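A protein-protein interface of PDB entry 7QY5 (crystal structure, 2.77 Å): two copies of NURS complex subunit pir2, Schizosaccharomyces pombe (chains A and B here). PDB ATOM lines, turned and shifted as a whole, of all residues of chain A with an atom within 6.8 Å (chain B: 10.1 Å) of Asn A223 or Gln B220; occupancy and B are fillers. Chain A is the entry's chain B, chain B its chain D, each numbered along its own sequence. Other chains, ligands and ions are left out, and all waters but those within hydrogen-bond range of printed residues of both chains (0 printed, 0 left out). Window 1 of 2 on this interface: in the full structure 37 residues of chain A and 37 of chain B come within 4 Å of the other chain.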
ATOM      1  N   VAL A 218     -20.798 -25.321   0.373  1.00  0.00           N
ATOM      2  CA  VAL A 218     -21.502 -24.255   1.152  1.00  0.00           C
ATOM      3  C   VAL A 218     -20.753 -24.095   2.489  1.00  0.00           C
ATOM      4  O   VAL A 218     -21.304 -24.523   3.530  1.00  0.00           O
ATOM      5  CB  VAL A 218     -23.003 -24.588   1.343  1.00  0.00           C
ATOM      6  CG1 VAL A 218     -23.839 -23.350   1.655  1.00  0.00           C
ATOM      7  CG2 VAL A 218     -23.589 -25.332   0.147  1.00  0.00           C
ATOM      8  N   GLY A 219     -19.526 -23.545   2.443  1.00  0.00           N
ATOM      9  CA  GLY A 219     -18.649 -23.237   3.596  1.00  0.00           C
ATOM     10  C   GLY A 219     -18.904 -24.161   4.776  1.00  0.00           C
ATOM     11  O   GLY A 219     -19.162 -23.644   5.885  1.00  0.00           O
ATOM     12  N   GLN A 220     -18.838 -25.477   4.540  1.00  0.00           N
ATOM     13  CA  GLN A 220     -19.216 -26.533   5.517  1.00  0.00           C
ATOM     14  C   GLN A 220     -18.522 -26.235   6.852  1.00  0.00           C
ATOM     15  O   GLN A 220     -19.176 -26.320   7.905  1.00  0.00           O
ATOM     16  CB  GLN A 220     -18.865 -27.919   4.971  1.00  0.00           C
ATOM     17  CG  GLN A 220     -19.580 -29.059   5.692  1.00  0.00           C
ATOM     18  CD  GLN A 220     -19.256 -30.434   5.145  1.00  0.00           C
ATOM     19  OE1 GLN A 220     -18.300 -30.626   4.392  1.00  0.00           O
ATOM     20  NE2 GLN A 220     -20.054 -31.416   5.539  1.00  0.00           N
ATOM     21  N   GLU A 221     -17.254 -25.843   6.810  1.00  0.00           N
ATOM     22  CA  GLU A 221     -16.488 -25.530   8.039  1.00  0.00           C
ATOM     23  C   GLU A 221     -17.235 -24.454   8.830  1.00  0.00           C
ATOM     24  O   GLU A 221     -17.398 -24.630  10.045  1.00  0.00           O
ATOM     25  CB  GLU A 221     -15.068 -25.100   7.682  1.00  0.00           C
ATOM     26  CG  GLU A 221     -14.417 -26.041   6.685  1.00  0.00           C
ATOM     27  CD  GLU A 221     -12.911 -26.184   6.799  1.00  0.00           C
ATOM     28  OE1 GLU A 221     -12.268 -25.305   7.432  1.00  0.00           O
ATOM     29  OE2 GLU A 221     -12.387 -27.180   6.246  1.00  0.00           O
ATOM     30  N   GLU A 222     -17.698 -23.404   8.150  1.00  0.00           N
ATOM     31  CA  GLU A 222     -18.308 -22.203   8.780  1.00  0.00           C
ATOM     32  C   GLU A 222     -19.604 -22.610   9.482  1.00  0.00           C
ATOM     33  O   GLU A 222     -19.786 -22.264  10.656  1.00  0.00           O
ATOM     34  CB  GLU A 222     -18.570 -21.110   7.746  1.00  0.00           C
ATOM     35  CG  GLU A 222     -17.346 -20.755   6.927  1.00  0.00           C
ATOM     36  CD  GLU A 222     -17.442 -19.392   6.275  1.00  0.00           C
ATOM     37  OE1 GLU A 222     -16.402 -18.903   5.771  1.00  0.00           O
ATOM     38  OE2 GLU A 222     -18.556 -18.821   6.289  1.00  0.00           O
ATOM     39  N   ASN A 223     -20.458 -23.361   8.800  1.00  0.00           N
ATOM     40  CA  ASN A 223     -21.766 -23.772   9.368  1.00  0.00           C
ATOM     41  C   ASN A 223     -21.513 -24.662  10.589  1.00  0.00           C
ATOM     42  O   ASN A 223     -22.316 -24.591  11.542  1.00  0.00           O
ATOM     43  CB  ASN A 223     -22.634 -24.392   8.280  1.00  0.00           C
ATOM     44  CG  ASN A 223     -22.789 -23.444   7.110  1.00  0.00           C
ATOM     45  OD1 ASN A 223     -22.113 -23.581   6.097  1.00  0.00           O
ATOM     46  ND2 ASN A 223     -23.617 -22.429   7.269  1.00  0.00           N
ATOM     47  N   ILE A 224     -20.416 -25.426  10.577  1.00  0.00           N
ATOM     48  CA  ILE A 224     -19.981 -26.308  11.702  1.00  0.00           C
ATOM     49  C   ILE A 224     -19.559 -25.434  12.881  1.00  0.00           C
ATOM     50  O   ILE A 224     -20.138 -25.583  13.969  1.00  0.00           O
ATOM     51  CB  ILE A 224     -18.861 -27.265  11.246  1.00  0.00           C
ATOM     52  CG1 ILE A 224     -19.450 -28.467  10.502  1.00  0.00           C
ATOM     53  CG2 ILE A 224     -17.985 -27.701  12.412  1.00  0.00           C
ATOM     54  CD1 ILE A 224     -18.459 -29.198   9.641  1.00  0.00           C
ATOM     55  N   TRP A 225     -18.569 -24.572  12.663  1.00  0.00           N
ATOM     56  CA  TRP A 225     -18.017 -23.674  13.707  1.00  0.00           C
ATOM     57  C   TRP A 225     -19.181 -22.991  14.409  1.00  0.00           C
ATOM     58  O   TRP A 225     -19.213 -23.023  15.649  1.00  0.00           O
ATOM     59  CB  TRP A 225     -17.061 -22.659  13.090  1.00  0.00           C
ATOM     60  CG  TRP A 225     -16.750 -21.506  13.989  1.00  0.00           C
ATOM     61  CD1 TRP A 225     -15.802 -21.456  14.966  1.00  0.00           C
ATOM     62  CD2 TRP A 225     -17.389 -20.219  13.987  1.00  0.00           C
ATOM     63  NE1 TRP A 225     -15.800 -20.225  15.565  1.00  0.00           N
ATOM     64  CE2 TRP A 225     -16.764 -19.448  14.991  1.00  0.00           C
ATOM     65  CE3 TRP A 225     -18.423 -19.652  13.239  1.00  0.00           C
ATOM     66  CZ2 TRP A 225     -17.140 -18.141  15.269  1.00  0.00           C
ATOM     67  CZ3 TRP A 225     -18.798 -18.358  13.512  1.00  0.00           C
ATOM     68  CH2 TRP A 225     -18.160 -17.615  14.510  1.00  0.00           C
ATOM     69  N   LEU A 226     -20.095 -22.429  13.617  1.00  0.00           N
ATOM     70  CA  LEU A 226     -21.267 -21.659  14.107  1.00  0.00           C
ATOM     71  C   LEU A 226     -22.178 -22.602  14.889  1.00  0.00           C
ATOM     72  O   LEU A 226     -22.615 -22.238  16.008  1.00  0.00           O
ATOM     73  CB  LEU A 226     -22.011 -21.024  12.928  1.00  0.00           C
ATOM     74  CG  LEU A 226     -23.288 -20.255  13.286  1.00  0.00           C
ATOM     75  CD1 LEU A 226     -23.040 -19.261  14.418  1.00  0.00           C
ATOM     76  CD2 LEU A 226     -23.877 -19.534  12.069  1.00  0.00           C
ATOM     77  N   SER A 227     -22.449 -23.768  14.315  1.00  0.00           N
ATOM     78  CA  SER A 227     -23.257 -24.823  14.961  1.00  0.00           C
ATOM     79  C   SER A 227     -22.638 -25.138  16.324  1.00  0.00           C
ATOM     80  O   SER A 227     -23.332 -24.989  17.342  1.00  0.00           O
ATOM     81  CB  SER A 227     -23.350 -26.035  14.096  1.00  0.00           C
ATOM     82  OG  SER A 227     -23.981 -27.080  14.813  1.00  0.00           O
ATOM     83  N   ASP A 228     -21.362 -25.525  16.334  1.00  0.00           N
ATOM     84  CA  ASP A 228     -20.629 -25.910  17.566  1.00  0.00           C
ATOM     85  C   ASP A 228     -20.750 -24.768  18.578  1.00  0.00           C
ATOM     86  O   ASP A 228     -21.027 -25.047  19.775  1.00  0.00           O
ATOM     87  CB  ASP A 228     -19.174 -26.267  17.253  1.00  0.00           C
ATOM     88  CG  ASP A 228     -18.930 -27.743  16.950  1.00  0.00           C
ATOM     89  OD1 ASP A 228     -19.913 -28.456  16.560  1.00  0.00           O
ATOM     90  OD2 ASP A 228     -17.756 -28.182  17.120  1.00  0.00           O
ATOM     91  N   PHE B 109     -14.951 -16.426  11.112  1.00  0.00           N
ATOM     92  CA  PHE B 109     -15.464 -16.818   9.777  1.00  0.00           C
ATOM     93  C   PHE B 109     -16.349 -15.728   9.168  1.00  0.00           C
ATOM     94  O   PHE B 109     -17.000 -14.925   9.887  1.00  0.00           O
ATOM     95  CB  PHE B 109     -16.249 -18.125   9.848  1.00  0.00           C
ATOM     96  CG  PHE B 109     -15.388 -19.352   9.821  1.00  0.00           C
ATOM     97  CD1 PHE B 109     -14.430 -19.510   8.833  1.00  0.00           C
ATOM     98  CD2 PHE B 109     -15.539 -20.339  10.778  1.00  0.00           C
ATOM     99  CE1 PHE B 109     -13.623 -20.632   8.811  1.00  0.00           C
ATOM    100  CE2 PHE B 109     -14.740 -21.471  10.747  1.00  0.00           C
ATOM    101  CZ  PHE B 109     -13.785 -21.614   9.763  1.00  0.00           C
ATOM    102  N   GLU B 110     -16.351 -15.731   7.834  1.00  0.00           N
ATOM    103  CA  GLU B 110     -17.261 -14.946   6.963  1.00  0.00           C
ATOM    104  C   GLU B 110     -18.632 -14.875   7.654  1.00  0.00           C
ATOM    105  O   GLU B 110     -19.060 -13.782   8.009  1.00  0.00           O
ATOM    106  CB  GLU B 110     -17.273 -15.605   5.576  1.00  0.00           C
ATOM    107  CG  GLU B 110     -17.584 -14.660   4.425  1.00  0.00           C
ATOM    108  CD  GLU B 110     -17.519 -15.276   3.028  1.00  0.00           C
ATOM    109  OE1 GLU B 110     -18.507 -15.141   2.247  1.00  0.00           O
ATOM    110  OE2 GLU B 110     -16.470 -15.881   2.708  1.00  0.00           O
ATOM    111  N   ILE B 111     -19.221 -16.034   7.942  1.00  0.00           N
ATOM    112  CA  ILE B 111     -20.659 -16.228   8.306  1.00  0.00           C
ATOM    113  C   ILE B 111     -21.073 -15.348   9.493  1.00  0.00           C
ATOM    114  O   ILE B 111     -22.242 -14.971   9.536  1.00  0.00           O
ATOM    115  CB  ILE B 111     -20.957 -17.716   8.579  1.00  0.00           C
ATOM    116  CG1 ILE B 111     -22.467 -17.959   8.647  1.00  0.00           C
ATOM    117  CG2 ILE B 111     -20.240 -18.199   9.832  1.00  0.00           C
ATOM    118  CD1 ILE B 111     -22.880 -19.420   8.723  1.00  0.00           C
ATOM    119  N   ALA B 112     -20.170 -15.044  10.426  1.00  0.00           N
ATOM    120  CA  ALA B 112     -20.462 -14.276  11.669  1.00  0.00           C
ATOM    121  C   ALA B 112     -20.833 -12.822  11.352  1.00  0.00           C
ATOM    122  O   ALA B 112     -21.259 -12.092  12.295  1.00  0.00           O
ATOM    123  CB  ALA B 112     -19.276 -14.311  12.602  1.00  0.00           C
ATOM    124  N   SER B 114     -22.735 -11.914   8.472  1.00  0.00           N
ATOM    125  CA  SER B 114     -23.911 -11.987   7.562  1.00  0.00           C
ATOM    126  C   SER B 114     -25.184 -11.551   8.287  1.00  0.00           C
ATOM    127  O   SER B 114     -25.296 -11.812   9.473  1.00  0.00           O
ATOM    128  CB  SER B 114     -24.080 -13.376   7.044  1.00  0.00           C
ATOM    129  OG  SER B 114     -24.652 -14.198   8.045  1.00  0.00           O
ATOM    130  N   GLN B 116     -28.424 -12.546   8.549  1.00  0.00           N
ATOM    131  CA  GLN B 116     -29.085 -13.619   9.326  1.00  0.00           C
ATOM    132  C   GLN B 116     -28.314 -13.863  10.635  1.00  0.00           C
ATOM    133  O   GLN B 116     -28.902 -13.707  11.723  1.00  0.00           O
ATOM    134  CB  GLN B 116     -29.168 -14.849   8.422  1.00  0.00           C
ATOM    135  CG  GLN B 116     -29.501 -16.150   9.141  1.00  0.00           C
ATOM    136  CD  GLN B 116     -30.917 -16.161   9.653  1.00  0.00           C
ATOM    137  OE1 GLN B 116     -31.228 -15.550  10.675  1.00  0.00           O
ATOM    138  NE2 GLN B 116     -31.781 -16.860   8.934  1.00  0.00           N
ATOM    139  N   THR B 117     -27.036 -14.225  10.535  1.00  0.00           N
ATOM    140  CA  THR B 117     -26.228 -14.798  11.650  1.00  0.00           C
ATOM    141  C   THR B 117     -25.892 -13.733  12.697  1.00  0.00           C
ATOM    142  O   THR B 117     -26.104 -13.986  13.894  1.00  0.00           O
ATOM    143  CB  THR B 117     -24.957 -15.453  11.106  1.00  0.00           C
ATOM    144  OG1 THR B 117     -25.428 -16.631  10.446  1.00  0.00           O
ATOM    145  CG2 THR B 117     -23.938 -15.773  12.177  1.00  0.00           C
ATOM    146  N   PHE B 212     -18.001 -10.530   4.617  1.00  0.00           N
ATOM    147  CA  PHE B 212     -19.073 -11.359   4.008  1.00  0.00           C
ATOM    148  C   PHE B 212     -19.303 -10.938   2.548  1.00  0.00           C
ATOM    149  O   PHE B 212     -19.600  -9.760   2.316  1.00  0.00           O
ATOM    150  CB  PHE B 212     -20.356 -11.233   4.830  1.00  0.00           C
ATOM    151  CG  PHE B 212     -21.439 -12.189   4.410  1.00  0.00           C
ATOM    152  CD1 PHE B 212     -22.598 -11.734   3.799  1.00  0.00           C
ATOM    153  CD2 PHE B 212     -21.276 -13.553   4.601  1.00  0.00           C
ATOM    154  CE1 PHE B 212     -23.582 -12.628   3.408  1.00  0.00           C
ATOM    155  CE2 PHE B 212     -22.257 -14.447   4.204  1.00  0.00           C
ATOM    156  CZ  PHE B 212     -23.411 -13.982   3.614  1.00  0.00           C
ATOM    157  N   LYS B 216     -20.613 -14.750  -2.933  1.00  0.00           N
ATOM    158  CA  LYS B 216     -20.214 -16.120  -2.500  1.00  0.00           C
ATOM    159  C   LYS B 216     -21.169 -16.639  -1.416  1.00  0.00           C
ATOM    160  O   LYS B 216     -20.734 -17.505  -0.633  1.00  0.00           O
ATOM    161  CB  LYS B 216     -18.766 -16.115  -2.003  1.00  0.00           C
ATOM    162  CG  LYS B 216     -17.743 -15.784  -3.080  1.00  0.00           C
ATOM    163  CD  LYS B 216     -16.330 -15.797  -2.579  1.00  0.00           C
ATOM    164  CE  LYS B 216     -15.318 -15.541  -3.672  1.00  0.00           C
ATOM    165  NZ  LYS B 216     -13.948 -15.448  -3.118  1.00  0.00           N
ATOM    166  N   GLU B 217     -22.420 -16.157  -1.406  1.00  0.00           N
ATOM    167  CA  GLU B 217     -23.463 -16.463  -0.385  1.00  0.00           C
ATOM    168  C   GLU B 217     -23.930 -17.920  -0.518  1.00  0.00           C
ATOM    169  O   GLU B 217     -24.272 -18.519   0.517  1.00  0.00           O
ATOM    170  CB  GLU B 217     -24.653 -15.502  -0.501  1.00  0.00           C
ATOM    171  CG  GLU B 217     -24.474 -14.221   0.299  1.00  0.00           C
ATOM    172  CD  GLU B 217     -25.702 -13.331   0.435  1.00  0.00           C
ATOM    173  OE1 GLU B 217     -26.047 -12.650  -0.543  1.00  0.00           O
ATOM    174  OE2 GLU B 217     -26.310 -13.311   1.525  1.00  0.00           O
ATOM    175  N   VAL B 218     -23.951 -18.472  -1.733  1.00  0.00           N
ATOM    176  CA  VAL B 218     -24.359 -19.886  -1.992  1.00  0.00           C
ATOM    177  C   VAL B 218     -25.835 -20.050  -1.625  1.00  0.00           C
ATOM    178  O   VAL B 218     -26.656 -19.819  -2.518  1.00  0.00           O
ATOM    179  CB  VAL B 218     -23.503 -20.883  -1.194  1.00  0.00           C
ATOM    180  CG1 VAL B 218     -23.730 -22.298  -1.691  1.00  0.00           C
ATOM    181  CG2 VAL B 218     -22.023 -20.532  -1.221  1.00  0.00           C
ATOM    182  N   GLN B 220     -28.765 -21.234   0.729  1.00  0.00           N
ATOM    183  CA  GLN B 220     -29.133 -22.124   1.863  1.00  0.00           C
ATOM    184  C   GLN B 220     -30.567 -22.672   1.714  1.00  0.00           C
ATOM    185  O   GLN B 220     -31.051 -23.304   2.670  1.00  0.00           O
ATOM    186  CB  GLN B 220     -28.998 -21.377   3.198  1.00  0.00           C
ATOM    187  CG  GLN B 220     -28.350 -22.211   4.308  1.00  0.00           C
ATOM    188  CD  GLN B 220     -26.864 -21.980   4.480  1.00  0.00           C
ATOM    189  OE1 GLN B 220     -26.439 -21.079   5.198  1.00  0.00           O
ATOM    190  NE2 GLN B 220     -26.047 -22.806   3.841  1.00  0.00           N
ATOM    191  N   GLU B 221     -31.242 -22.469   0.581  1.00  0.00           N
ATOM    192  CA  GLU B 221     -32.595 -23.036   0.363  1.00  0.00           C
ATOM    193  C   GLU B 221     -32.552 -24.539   0.644  1.00  0.00           C
ATOM    194  O   GLU B 221     -33.405 -25.031   1.400  1.00  0.00           O
ATOM    195  CB  GLU B 221     -33.053 -22.782  -1.069  1.00  0.00           C
ATOM    196  CG  GLU B 221     -33.350 -21.322  -1.351  1.00  0.00           C
ATOM    197  CD  GLU B 221     -34.156 -21.078  -2.615  1.00  0.00           C
ATOM    198  OE1 GLU B 221     -34.560 -19.907  -2.838  1.00  0.00           O
ATOM    199  OE2 GLU B 221     -34.393 -22.060  -3.368  1.00  0.00           O
ATOM    200  N   GLU B 222     -31.556 -25.222   0.074  1.00  0.00           N
ATOM    201  CA  GLU B 222     -31.357 -26.693   0.171  1.00  0.00           C
ATOM    202  C   GLU B 222     -31.293 -27.117   1.633  1.00  0.00           C
ATOM    203  O   GLU B 222     -31.816 -28.178   1.975  1.00  0.00           O
ATOM    204  CB  GLU B 222     -30.060 -27.116  -0.510  1.00  0.00           C
ATOM    205  CG  GLU B 222     -30.007 -26.715  -1.969  1.00  0.00           C
ATOM    206  CD  GLU B 222     -28.989 -27.466  -2.803  1.00  0.00           C
ATOM    207  OE1 GLU B 222     -28.777 -27.063  -3.969  1.00  0.00           O
ATOM    208  OE2 GLU B 222     -28.416 -28.453  -2.286  1.00  0.00           O
ATOM    209  N   ASN B 223     -30.672 -26.301   2.467  1.00  0.00           N
ATOM    210  CA  ASN B 223     -30.430 -26.654   3.886  1.00  0.00           C
ATOM    211  C   ASN B 223     -31.702 -26.360   4.683  1.00  0.00           C
ATOM    212  O   ASN B 223     -31.945 -27.081   5.660  1.00  0.00           O
ATOM    213  CB  ASN B 223     -29.185 -25.950   4.413  1.00  0.00           C
ATOM    214  CG  ASN B 223     -28.008 -26.139   3.481  1.00  0.00           C
ATOM    215  OD1 ASN B 223     -27.110 -26.924   3.769  1.00  0.00           O
ATOM    216  ND2 ASN B 223     -28.036 -25.464   2.338  1.00  0.00           N
ATOM    217  N   ILE B 224     -32.481 -25.352   4.280  1.00  0.00           N
ATOM    218  CA  ILE B 224     -33.839 -25.096   4.843  1.00  0.00           C
ATOM    219  C   ILE B 224     -34.713 -26.308   4.520  1.00  0.00           C
ATOM    220  O   ILE B 224     -35.206 -26.974   5.450  1.00  0.00           O
ATOM    221  CB  ILE B 224     -34.429 -23.792   4.290  1.00  0.00           C
ATOM    222  CG1 ILE B 224     -33.831 -22.589   5.022  1.00  0.00           C
ATOM    223  CG2 ILE B 224     -35.948 -23.799   4.350  1.00  0.00           C
ATOM    224  CD1 ILE B 224     -33.974 -21.271   4.285  1.00  0.00           C
ATOM    225  N   TRP B 225     -34.868 -26.601   3.237  1.00  0.00           N
ATOM    226  CA  TRP B 225     -35.657 -27.766   2.773  1.00  0.00           C
ATOM    227  C   TRP B 225     -35.321 -29.011   3.609  1.00  0.00           C
ATOM    228  O   TRP B 225     -36.243 -29.657   4.148  1.00  0.00           O
ATOM    229  CB  TRP B 225     -35.402 -27.997   1.285  1.00  0.00           C
ATOM    230  CG  TRP B 225     -35.962 -29.301   0.830  1.00  0.00           C
ATOM    231  CD1 TRP B 225     -37.274 -29.595   0.627  1.00  0.00           C
ATOM    232  CD2 TRP B 225     -35.232 -30.513   0.595  1.00  0.00           C
ATOM    233  NE1 TRP B 225     -37.408 -30.901   0.250  1.00  0.00           N
ATOM    234  CE2 TRP B 225     -36.174 -31.489   0.216  1.00  0.00           C
ATOM    235  CE3 TRP B 225     -33.883 -30.869   0.674  1.00  0.00           C
ATOM    236  CZ2 TRP B 225     -35.807 -32.790  -0.108  1.00  0.00           C
ATOM    237  CZ3 TRP B 225     -33.522 -32.159   0.361  1.00  0.00           C
ATOM    238  CH2 TRP B 225     -34.471 -33.104  -0.030  1.00  0.00           C
ATOM    239  N   LEU B 226     -34.041 -29.356   3.689  1.00  0.00           N
ATOM    240  CA  LEU B 226     -33.569 -30.546   4.434  1.00  0.00           C
ATOM    241  C   LEU B 226     -34.013 -30.408   5.890  1.00  0.00           C
ATOM    242  O   LEU B 226     -34.672 -31.337   6.391  1.00  0.00           O
ATOM    243  CB  LEU B 226     -32.046 -30.630   4.325  1.00  0.00           C
ATOM    244  CG  LEU B 226     -31.405 -31.838   5.008  1.00  0.00           C
ATOM    245  CD1 LEU B 226     -32.159 -33.129   4.677  1.00  0.00           C
ATOM    246  CD2 LEU B 226     -29.935 -31.962   4.616  1.00  0.00           C
ATOM    247  N   SER B 227     -33.669 -29.272   6.511  1.00  0.00           N
ATOM    248  CA  SER B 227     -33.958 -28.922   7.927  1.00  0.00           C
ATOM    249  C   SER B 227     -35.436 -29.187   8.212  1.00  0.00           C
ATOM    250  O   SER B 227     -35.729 -29.958   9.143  1.00  0.00           O
ATOM    251  CB  SER B 227     -33.596 -27.484   8.233  1.00  0.00           C
ATOM    252  OG  SER B 227     -34.284 -27.007   9.383  1.00  0.00           O
ATOM    253  N   ASP B 228     -36.321 -28.564   7.426  1.00  0.00           N
ATOM    254  CA  ASP B 228     -37.797 -28.669   7.594  1.00  0.00           C
ATOM    255  C   ASP B 228     -38.186 -30.139   7.443  1.00  0.00           C
ATOM    256  O   ASP B 228     -39.011 -30.630   8.248  1.00  0.00           O
ATOM    257  CB  ASP B 228     -38.544 -27.736   6.635  1.00  0.00           C
ATOM    258  CG  ASP B 228     -38.586 -26.288   7.109  1.00  0.00           C
ATOM    259  OD1 ASP B 228     -37.827 -25.934   8.070  1.00  0.00           O
ATOM    260  OD2 ASP B 228     -39.380 -25.511   6.522  1.00  0.00           O
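No residue of chain B comes within 4 Å of Gly A219. Asn A223 touches two residues of chain B. Of the printed residues of chain B, Trp A225 touches Phe B109 (3.5 Å), Ile B111 (3.96 Å) and Ala B112 (3.98 Å). Of the printed residues of chain A, Phe B109 touches Glu A222 and Trp A225. Of the printed residues of chain A, Ile B111 touches Glu A222 (3.3 Å), Asn A223 (3.4 Å), Trp A225 (3.96 Å) and Leu A226 (3.5 Å). Of the printed residues of chain A, Val B218 touches Val A218. Of chain A, only Val A218 (3.2 Å) and Asn A223 (3.8 Å) come within 4 Å of Gln B220. The nearest residue of chain A that does not touch Gln B220 is Gly A219 (6.7 Å).
Among the printed residues, merely in contact across the chains: Val A218 with Gln B220, Glu A222 with Glu B110, Asn A223 with Ile B111, Leu A226 with Ile B111, Trp A225 with Phe B109, Val A218 with Val B218, Leu A226 with Thr B117, Glu A222 with Phe B109, Asn A223 with Gln B220, Trp A225 with Ile B111 and Trp A225 with Ala B112.
The side-chain amide oxygen (OD1) of Asn A223 sits close to the backbone carbonyl oxygen (O) of Val A218. The backbone carbonyl oxygen (O) of Gly A219 lies close to the side-chain amide oxygen (OD1) of Asn A223. The backbone carbonyl oxygen (O) of Ile B111 sits at hydrogen-bond distance from the side-chain hydroxyl (OG) of Ser B114, 2.9 Å away. The side-chain hydroxyl of Ser B114 lies close to the backbone NH of Thr B117 (3.4 Å).
OE2 of Glu A222 sits at hydrogen-bond distance from N of Ile B111 (3.3 Å).
Val B218 touches its own counterpart, Val A218. Val A218 touches Gln B220, but with the chains exchanged Gln A220 does not touch Val B218 (8.2 Å). Asn A223 touches Gln B220, but with the chains exchanged Gln A220 does not touch Asn B223 (8.1 Å). Positions printed for both chains: 218, 220, 221, 222, 223, 224, 225, 226, 227 and 228.
Printed residues of chain B that touch a printed residue of chain A: Phe B109, Glu B110, Ile B111, Ala B112, Thr B117, Val B218 and Gln B220. Among the printed residues, no Asp or Glu carboxylate lies within 4 Å of a Lys or Arg side-chain nitrogen of the other chain.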
